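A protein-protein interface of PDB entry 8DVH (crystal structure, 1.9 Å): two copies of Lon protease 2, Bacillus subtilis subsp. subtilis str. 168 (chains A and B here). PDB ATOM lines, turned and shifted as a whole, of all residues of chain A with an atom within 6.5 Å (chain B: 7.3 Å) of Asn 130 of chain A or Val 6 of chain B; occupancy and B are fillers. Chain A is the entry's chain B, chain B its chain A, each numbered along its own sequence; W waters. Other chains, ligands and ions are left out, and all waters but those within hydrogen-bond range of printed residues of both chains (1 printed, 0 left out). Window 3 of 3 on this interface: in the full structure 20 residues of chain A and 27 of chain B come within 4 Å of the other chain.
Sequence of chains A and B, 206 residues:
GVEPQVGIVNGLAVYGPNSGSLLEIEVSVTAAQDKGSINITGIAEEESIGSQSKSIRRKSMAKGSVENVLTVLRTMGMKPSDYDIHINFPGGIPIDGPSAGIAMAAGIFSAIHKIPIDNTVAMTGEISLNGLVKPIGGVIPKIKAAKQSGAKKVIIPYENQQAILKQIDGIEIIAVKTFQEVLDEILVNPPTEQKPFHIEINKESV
Water W1 lies within hydrogen-bond range of ND2 of Asn 88 of chain B (2.9 Å) and O of Ile 127 of chain A (2.9 Å).
Among the printed residues, pairs that only touch across the chains: Thr 71 of chain A with Ser 28 of chain B (3.6 Å), Ser 128 of chain A with Glu 26 of chain B (3.3 Å), Leu 129 of chain A with Val 6 of chain B (3.4 Å), Leu 129 of chain A with Ser 28 of chain B (3.96 Å), Leu 129 of chain A with His 86 of chain B (3.4 Å), Leu 129 of chain A with Asn 88 of chain B (3.7 Å) and Asn 130 of chain A with Val 6 of chain B (3.8 Å).
No position is printed for both chains.
Of the printed residues of chain B, Thr 71 of chain A touches Ser 28 and His 86.
Val 72 of chain A touches none of the printed residues of chain B.
Lys 134 of chain A touches none of the printed residues of chain B.
Of the printed residues of chain A, His 86 of chain B touches Thr 71 (2.9 Å) and Leu 129 (3.4 Å).
Of the printed residues of chain A, Asn 88 of chain B touches Leu 129 (3.7 Å).
The nearest residue of chain B that does not touch Asn 130 of chain A is Ile 8 of chain B (4.03 Å).
The nearest residue of chain A that does not touch Val 6 of chain B is Thr 75 of chain A (4.2 Å).
The nearest printed residue of chain A that does not touch Ser 28 of chain B is Thr 75 of chain A (4.8 Å).
The side-chain carboxylate of Glu 26 of chain B sits at hydrogen-bond distance from the backbone NH of Leu 129 of chain A (2.9 Å).
ND1 of His 86 of chain B lies within hydrogen-bond range of OG1 of Thr 71 of chain A (2.9 Å).
Printed residues of chain B that touch a printed residue of chain A: Val 6, Glu 26, Ser 28, His 86 and Asn 88.
Among the printed residues, 9 pairs touch across the chains.
The side-chain carboxylate (OE1) of Glu 26 of chain B sits at hydrogen-bond distance from the side-chain amide nitrogen (ND2) of Asn 88 of chain B (2.8 Å).
N of Ser 28 of chain B lies within hydrogen-bond range of O of His 86 of chain B (2.8 Å).
The side-chain hydroxyl of Ser 128 of chain A is in hydrogen-bond range of the side-chain amide oxygen of Asn 130 of chain A (2.4 Å).
OG of Ser 128 of chain A is in hydrogen-bond range of N of Leu 132 of chain A (3.1 Å).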
ATOM      1  N   THR A  71      -4.668   0.149 -24.830  1.00  0.00           N
ATOM      2  CA  THR A  71      -5.549   1.246 -24.367  1.00  0.00           C
ATOM      3  C   THR A  71      -5.357   1.458 -22.854  1.00  0.00           C
ATOM      4  O   THR A  71      -5.170   2.598 -22.454  1.00  0.00           O
ATOM      5  CB  THR A  71      -6.988   1.038 -24.811  1.00  0.00           C
ATOM      6  OG1 THR A  71      -6.961   1.188 -26.228  1.00  0.00           O
ATOM      7  CG2 THR A  71      -7.938   2.014 -24.135  1.00  0.00           C
ATOM      8  N   VAL A  72      -5.276   0.402 -22.045  1.00  0.00           N
ATOM      9  CA  VAL A  72      -5.085   0.541 -20.579  1.00  0.00           C
ATOM     10  C   VAL A  72      -3.739   1.227 -20.312  1.00  0.00           C
ATOM     11  O   VAL A  72      -3.725   2.173 -19.463  1.00  0.00           O
ATOM     12  CB  VAL A  72      -5.212  -0.804 -19.850  1.00  0.00           C
ATOM     13  CG1 VAL A  72      -4.783  -0.719 -18.394  1.00  0.00           C
ATOM     14  CG2 VAL A  72      -6.623  -1.344 -19.943  1.00  0.00           C
ATOM     15  N   THR A  75      -3.994   4.985 -20.722  1.00  0.00           N
ATOM     16  CA  THR A  75      -4.761   5.629 -19.616  1.00  0.00           C
ATOM     17  C   THR A  75      -3.858   5.760 -18.387  1.00  0.00           C
ATOM     18  O   THR A  75      -4.081   6.693 -17.590  1.00  0.00           O
ATOM     19  CB  THR A  75      -6.047   4.881 -19.242  1.00  0.00           C
ATOM     20  OG1 THR A  75      -5.709   3.668 -18.560  1.00  0.00           O
ATOM     21  CG2 THR A  75      -6.935   4.621 -20.439  1.00  0.00           C
ATOM     22  N   ILE A 127      -8.685  -8.305 -19.307  1.00  0.00           N
ATOM     23  CA  ILE A 127      -8.480  -6.896 -18.876  1.00  0.00           C
ATOM     24  C   ILE A 127      -9.547  -6.057 -19.569  1.00  0.00           C
ATOM     25  O   ILE A 127      -9.801  -6.277 -20.764  1.00  0.00           O
ATOM     26  CB  ILE A 127      -7.041  -6.390 -19.117  1.00  0.00           C
ATOM     27  CG1 ILE A 127      -6.758  -5.125 -18.317  1.00  0.00           C
ATOM     28  CG2 ILE A 127      -6.762  -6.131 -20.572  1.00  0.00           C
ATOM     29  CD1 ILE A 127      -5.340  -4.651 -18.416  1.00  0.00           C
ATOM     30  N   SER A 128     -10.191  -5.155 -18.835  1.00  0.00           N
ATOM     31  CA  SER A 128     -11.169  -4.204 -19.421  1.00  0.00           C
ATOM     32  C   SER A 128     -10.483  -2.860 -19.718  1.00  0.00           C
ATOM     33  O   SER A 128      -9.381  -2.659 -19.240  1.00  0.00           O
ATOM     34  CB  SER A 128     -12.348  -4.057 -18.507  1.00  0.00           C
ATOM     35  OG  SER A 128     -11.976  -3.310 -17.369  1.00  0.00           O
ATOM     36  N   LEU A 129     -11.119  -1.949 -20.459  1.00  0.00           N
ATOM     37  CA  LEU A 129     -10.445  -0.667 -20.842  1.00  0.00           C
ATOM     38  C   LEU A 129     -10.213   0.220 -19.608  1.00  0.00           C
ATOM     39  O   LEU A 129      -9.343   1.078 -19.669  1.00  0.00           O
ATOM     40  CB  LEU A 129     -11.276   0.074 -21.895  1.00  0.00           C
ATOM     41  CG  LEU A 129     -11.565  -0.621 -23.228  1.00  0.00           C
ATOM     42  CD1 LEU A 129     -12.142   0.395 -24.184  1.00  0.00           C
ATOM     43  CD2 LEU A 129     -10.345  -1.262 -23.879  1.00  0.00           C
ATOM     44  N   ASN A 130     -10.922  -0.034 -18.505  1.00  0.00           N
ATOM     45  CA  ASN A 130     -10.795   0.734 -17.235  1.00  0.00           C
ATOM     46  C   ASN A 130      -9.937  -0.061 -16.250  1.00  0.00           C
ATOM     47  O   ASN A 130     -10.029   0.238 -15.060  1.00  0.00           O
ATOM     48  CB  ASN A 130     -12.164   1.134 -16.657  1.00  0.00           C
ATOM     49  CG  ASN A 130     -13.175   0.005 -16.536  1.00  0.00           C
ATOM     50  OD1 ASN A 130     -12.865  -1.169 -16.702  1.00  0.00           O
ATOM     51  ND2 ASN A 130     -14.404   0.345 -16.195  1.00  0.00           N
ATOM     52  N   GLY A 131      -9.133  -1.026 -16.710  1.00  0.00           N
ATOM     53  CA  GLY A 131      -8.097  -1.653 -15.876  1.00  0.00           C
ATOM     54  C   GLY A 131      -8.666  -2.693 -14.924  1.00  0.00           C
ATOM     55  O   GLY A 131      -7.910  -3.220 -14.120  1.00  0.00           O
ATOM     56  N   LEU A 132      -9.948  -3.019 -15.015  1.00  0.00           N
ATOM     57  CA  LEU A 132     -10.556  -4.057 -14.148  1.00  0.00           C
ATOM     58  C   LEU A 132     -10.197  -5.437 -14.709  1.00  0.00           C
ATOM     59  O   LEU A 132      -9.987  -5.563 -15.918  1.00  0.00           O
ATOM     60  CB  LEU A 132     -12.062  -3.825 -14.063  1.00  0.00           C
ATOM     61  CG  LEU A 132     -12.466  -2.419 -13.592  1.00  0.00           C
ATOM     62  CD1 LEU A 132     -13.978  -2.331 -13.369  1.00  0.00           C
ATOM     63  CD2 LEU A 132     -11.722  -2.036 -12.325  1.00  0.00           C
ATOM     64  N   LYS A 134     -11.425  -9.138 -15.304  1.00  0.00           N
ATOM     65  CA  LYS A 134     -12.735  -9.759 -15.571  1.00  0.00           C
ATOM     66  C   LYS A 134     -12.557 -11.272 -15.481  1.00  0.00           C
ATOM     67  O   LYS A 134     -11.451 -11.768 -15.723  1.00  0.00           O
ATOM     68  CB  LYS A 134     -13.251  -9.282 -16.927  1.00  0.00           C
ATOM     69  CG  LYS A 134     -13.382  -7.761 -17.083  1.00  0.00           C
ATOM     70  CD  LYS A 134     -14.343  -7.161 -16.078  1.00  0.00           C
ATOM     71  CE  LYS A 134     -14.856  -5.770 -16.399  1.00  0.00           C
ATOM     72  NZ  LYS A 134     -15.863  -5.357 -15.391  1.00  0.00           N
ATOM     73  N   THR A 178      -8.163  -5.340 -10.039  1.00  0.00           N
ATOM     74  CA  THR A 178      -7.547  -4.301 -10.905  1.00  0.00           C
ATOM     75  C   THR A 178      -6.158  -4.722 -11.364  1.00  0.00           C
ATOM     76  O   THR A 178      -5.476  -5.521 -10.681  1.00  0.00           O
ATOM     77  CB  THR A 178      -7.481  -2.927 -10.224  1.00  0.00           C
ATOM     78  OG1 THR A 178      -6.404  -2.953  -9.282  1.00  0.00           O
ATOM     79  CG2 THR A 178      -8.783  -2.547  -9.557  1.00  0.00           C
ATOM     80  N   VAL B   6     -12.545   6.377 -18.864  1.00  0.00           N
ATOM     81  CA  VAL B   6     -13.213   5.251 -19.588  1.00  0.00           C
ATOM     82  C   VAL B   6     -14.663   5.120 -19.087  1.00  0.00           C
ATOM     83  O   VAL B   6     -14.875   4.730 -17.917  1.00  0.00           O
ATOM     84  CB  VAL B   6     -12.443   3.925 -19.417  1.00  0.00           C
ATOM     85  CG1 VAL B   6     -13.277   2.743 -19.910  1.00  0.00           C
ATOM     86  CG2 VAL B   6     -11.087   3.967 -20.111  1.00  0.00           C
ATOM     87  N   GLY B   7     -15.631   5.426 -19.942  1.00  0.00           N
ATOM     88  CA  GLY B   7     -17.053   5.477 -19.567  1.00  0.00           C
ATOM     89  C   GLY B   7     -17.746   4.168 -19.920  1.00  0.00           C
ATOM     90  O   GLY B   7     -17.230   3.408 -20.807  1.00  0.00           O
ATOM     91  N   ILE B   8     -18.861   3.911 -19.240  1.00  0.00           N
ATOM     92  CA  ILE B   8     -19.698   2.703 -19.410  1.00  0.00           C
ATOM     93  C   ILE B   8     -21.057   3.171 -19.921  1.00  0.00           C
ATOM     94  O   ILE B   8     -21.640   4.116 -19.355  1.00  0.00           O
ATOM     95  CB  ILE B   8     -19.839   1.898 -18.104  1.00  0.00           C
ATOM     96  CG1 ILE B   8     -18.491   1.449 -17.541  1.00  0.00           C
ATOM     97  CG2 ILE B   8     -20.773   0.717 -18.313  1.00  0.00           C
ATOM     98  CD1 ILE B   8     -17.784   0.424 -18.388  1.00  0.00           C
ATOM     99  N   ILE B  25     -20.932  -1.763 -21.974  1.00  0.00           N
ATOM    100  CA  ILE B  25     -20.054  -1.393 -23.108  1.00  0.00           C
ATOM    101  C   ILE B  25     -19.073  -0.335 -22.614  1.00  0.00           C
ATOM    102  O   ILE B  25     -19.534   0.682 -22.065  1.00  0.00           O
ATOM    103  CB  ILE B  25     -20.893  -0.878 -24.287  1.00  0.00           C
ATOM    104  CG1 ILE B  25     -21.913  -1.935 -24.722  1.00  0.00           C
ATOM    105  CG2 ILE B  25     -20.015  -0.390 -25.412  1.00  0.00           C
ATOM    106  CD1 ILE B  25     -23.010  -1.382 -25.534  1.00  0.00           C
ATOM    107  N   GLU B  26     -17.788  -0.541 -22.862  1.00  0.00           N
ATOM    108  CA  GLU B  26     -16.715   0.370 -22.396  1.00  0.00           C
ATOM    109  C   GLU B  26     -16.303   1.273 -23.557  1.00  0.00           C
ATOM    110  O   GLU B  26     -16.082   0.780 -24.697  1.00  0.00           O
ATOM    111  CB  GLU B  26     -15.531  -0.444 -21.872  1.00  0.00           C
ATOM    112  CG  GLU B  26     -15.883  -1.526 -20.861  1.00  0.00           C
ATOM    113  CD  GLU B  26     -14.905  -2.702 -20.696  1.00  0.00           C
ATOM    114  OE1 GLU B  26     -13.789  -2.708 -21.269  1.00  0.00           O
ATOM    115  OE2 GLU B  26     -15.292  -3.671 -19.989  1.00  0.00           O
ATOM    116  N   VAL B  27     -16.129   2.556 -23.281  1.00  0.00           N
ATOM    117  CA  VAL B  27     -15.791   3.530 -24.340  1.00  0.00           C
ATOM    118  C   VAL B  27     -14.630   4.365 -23.820  1.00  0.00           C
ATOM    119  O   VAL B  27     -14.792   4.992 -22.732  1.00  0.00           O
ATOM    120  CB  VAL B  27     -17.000   4.407 -24.714  1.00  0.00           C
ATOM    121  CG1 VAL B  27     -16.649   5.279 -25.898  1.00  0.00           C
ATOM    122  CG2 VAL B  27     -18.227   3.578 -25.034  1.00  0.00           C
ATOM    123  N   SER B  28     -13.490   4.250 -24.490  1.00  0.00           N
ATOM    124  CA  SER B  28     -12.284   5.059 -24.234  1.00  0.00           C
ATOM    125  C   SER B  28     -12.137   6.044 -25.380  1.00  0.00           C
ATOM    126  O   SER B  28     -12.170   5.621 -26.539  1.00  0.00           O
ATOM    127  CB  SER B  28     -11.056   4.207 -24.092  1.00  0.00           C
ATOM    128  OG  SER B  28      -9.894   5.017 -24.231  1.00  0.00           O
ATOM    129  N   VAL B  29     -11.987   7.326 -25.059  1.00  0.00           N
ATOM    130  CA  VAL B  29     -11.744   8.374 -26.071  1.00  0.00           C
ATOM    131  C   VAL B  29     -10.563   9.190 -25.540  1.00  0.00           C
ATOM    132  O   VAL B  29     -10.663   9.630 -24.403  1.00  0.00           O
ATOM    133  CB  VAL B  29     -13.001   9.238 -26.277  1.00  0.00           C
ATOM    134  CG1 VAL B  29     -12.696  10.484 -27.092  1.00  0.00           C
ATOM    135  CG2 VAL B  29     -14.136   8.459 -26.906  1.00  0.00           C
ATOM    136  N   THR B  30      -9.476   9.258 -26.292  1.00  0.00           N
ATOM    137  CA  THR B  30      -8.242  10.018 -25.938  1.00  0.00           C
ATOM    138  C   THR B  30      -7.875  10.908 -27.120  1.00  0.00           C
ATOM    139  O   THR B  30      -8.219  10.553 -28.254  1.00  0.00           O
ATOM    140  CB  THR B  30      -7.109   9.056 -25.550  1.00  0.00           C
ATOM    141  OG1 THR B  30      -6.940   8.103 -26.594  1.00  0.00           O
ATOM    142  CG2 THR B  30      -7.396   8.320 -24.263  1.00  0.00           C
ATOM    143  N   HIS B  86     -11.827   3.746 -28.700  1.00  0.00           N
ATOM    144  CA  HIS B  86     -11.838   2.278 -28.540  1.00  0.00           C
ATOM    145  C   HIS B  86     -13.098   1.940 -27.765  1.00  0.00           C
ATOM    146  O   HIS B  86     -13.274   2.433 -26.615  1.00  0.00           O
ATOM    147  CB  HIS B  86     -10.542   1.819 -27.878  1.00  0.00           C
ATOM    148  CG  HIS B  86     -10.393   0.344 -27.773  1.00  0.00           C
ATOM    149  ND1 HIS B  86      -9.242  -0.240 -27.302  1.00  0.00           N
ATOM    150  CD2 HIS B  86     -11.231  -0.674 -28.056  1.00  0.00           C
ATOM    151  CE1 HIS B  86      -9.375  -1.550 -27.311  1.00  0.00           C
ATOM    152  NE2 HIS B  86     -10.583  -1.841 -27.732  1.00  0.00           N
ATOM    153  N   ASN B  88     -15.146  -1.431 -26.347  1.00  0.00           N
ATOM    154  CA  ASN B  88     -14.961  -2.833 -25.968  1.00  0.00           C
ATOM    155  C   ASN B  88     -16.309  -3.380 -25.499  1.00  0.00           C
ATOM    156  O   ASN B  88     -16.905  -2.828 -24.560  1.00  0.00           O
ATOM    157  CB  ASN B  88     -13.873  -2.963 -24.908  1.00  0.00           C
ATOM    158  CG  ASN B  88     -13.598  -4.392 -24.551  1.00  0.00           C
ATOM    159  OD1 ASN B  88     -13.319  -5.186 -25.444  1.00  0.00           O
ATOM    160  ND2 ASN B  88     -13.662  -4.704 -23.275  1.00  0.00           N
ATOM    161  N   ALA B 111     -17.971  10.839 -23.536  1.00  0.00           N
ATOM    162  CA  ALA B 111     -16.502  10.808 -23.385  1.00  0.00           C
ATOM    163  C   ALA B 111     -15.893  12.108 -23.939  1.00  0.00           C
ATOM    164  O   ALA B 111     -15.038  12.730 -23.252  1.00  0.00           O
ATOM    165  CB  ALA B 111     -15.958   9.577 -24.055  1.00  0.00           C
HETATM  166  O   HOH W   1     -12.482  -6.754 -21.683  1.00  0.00           O
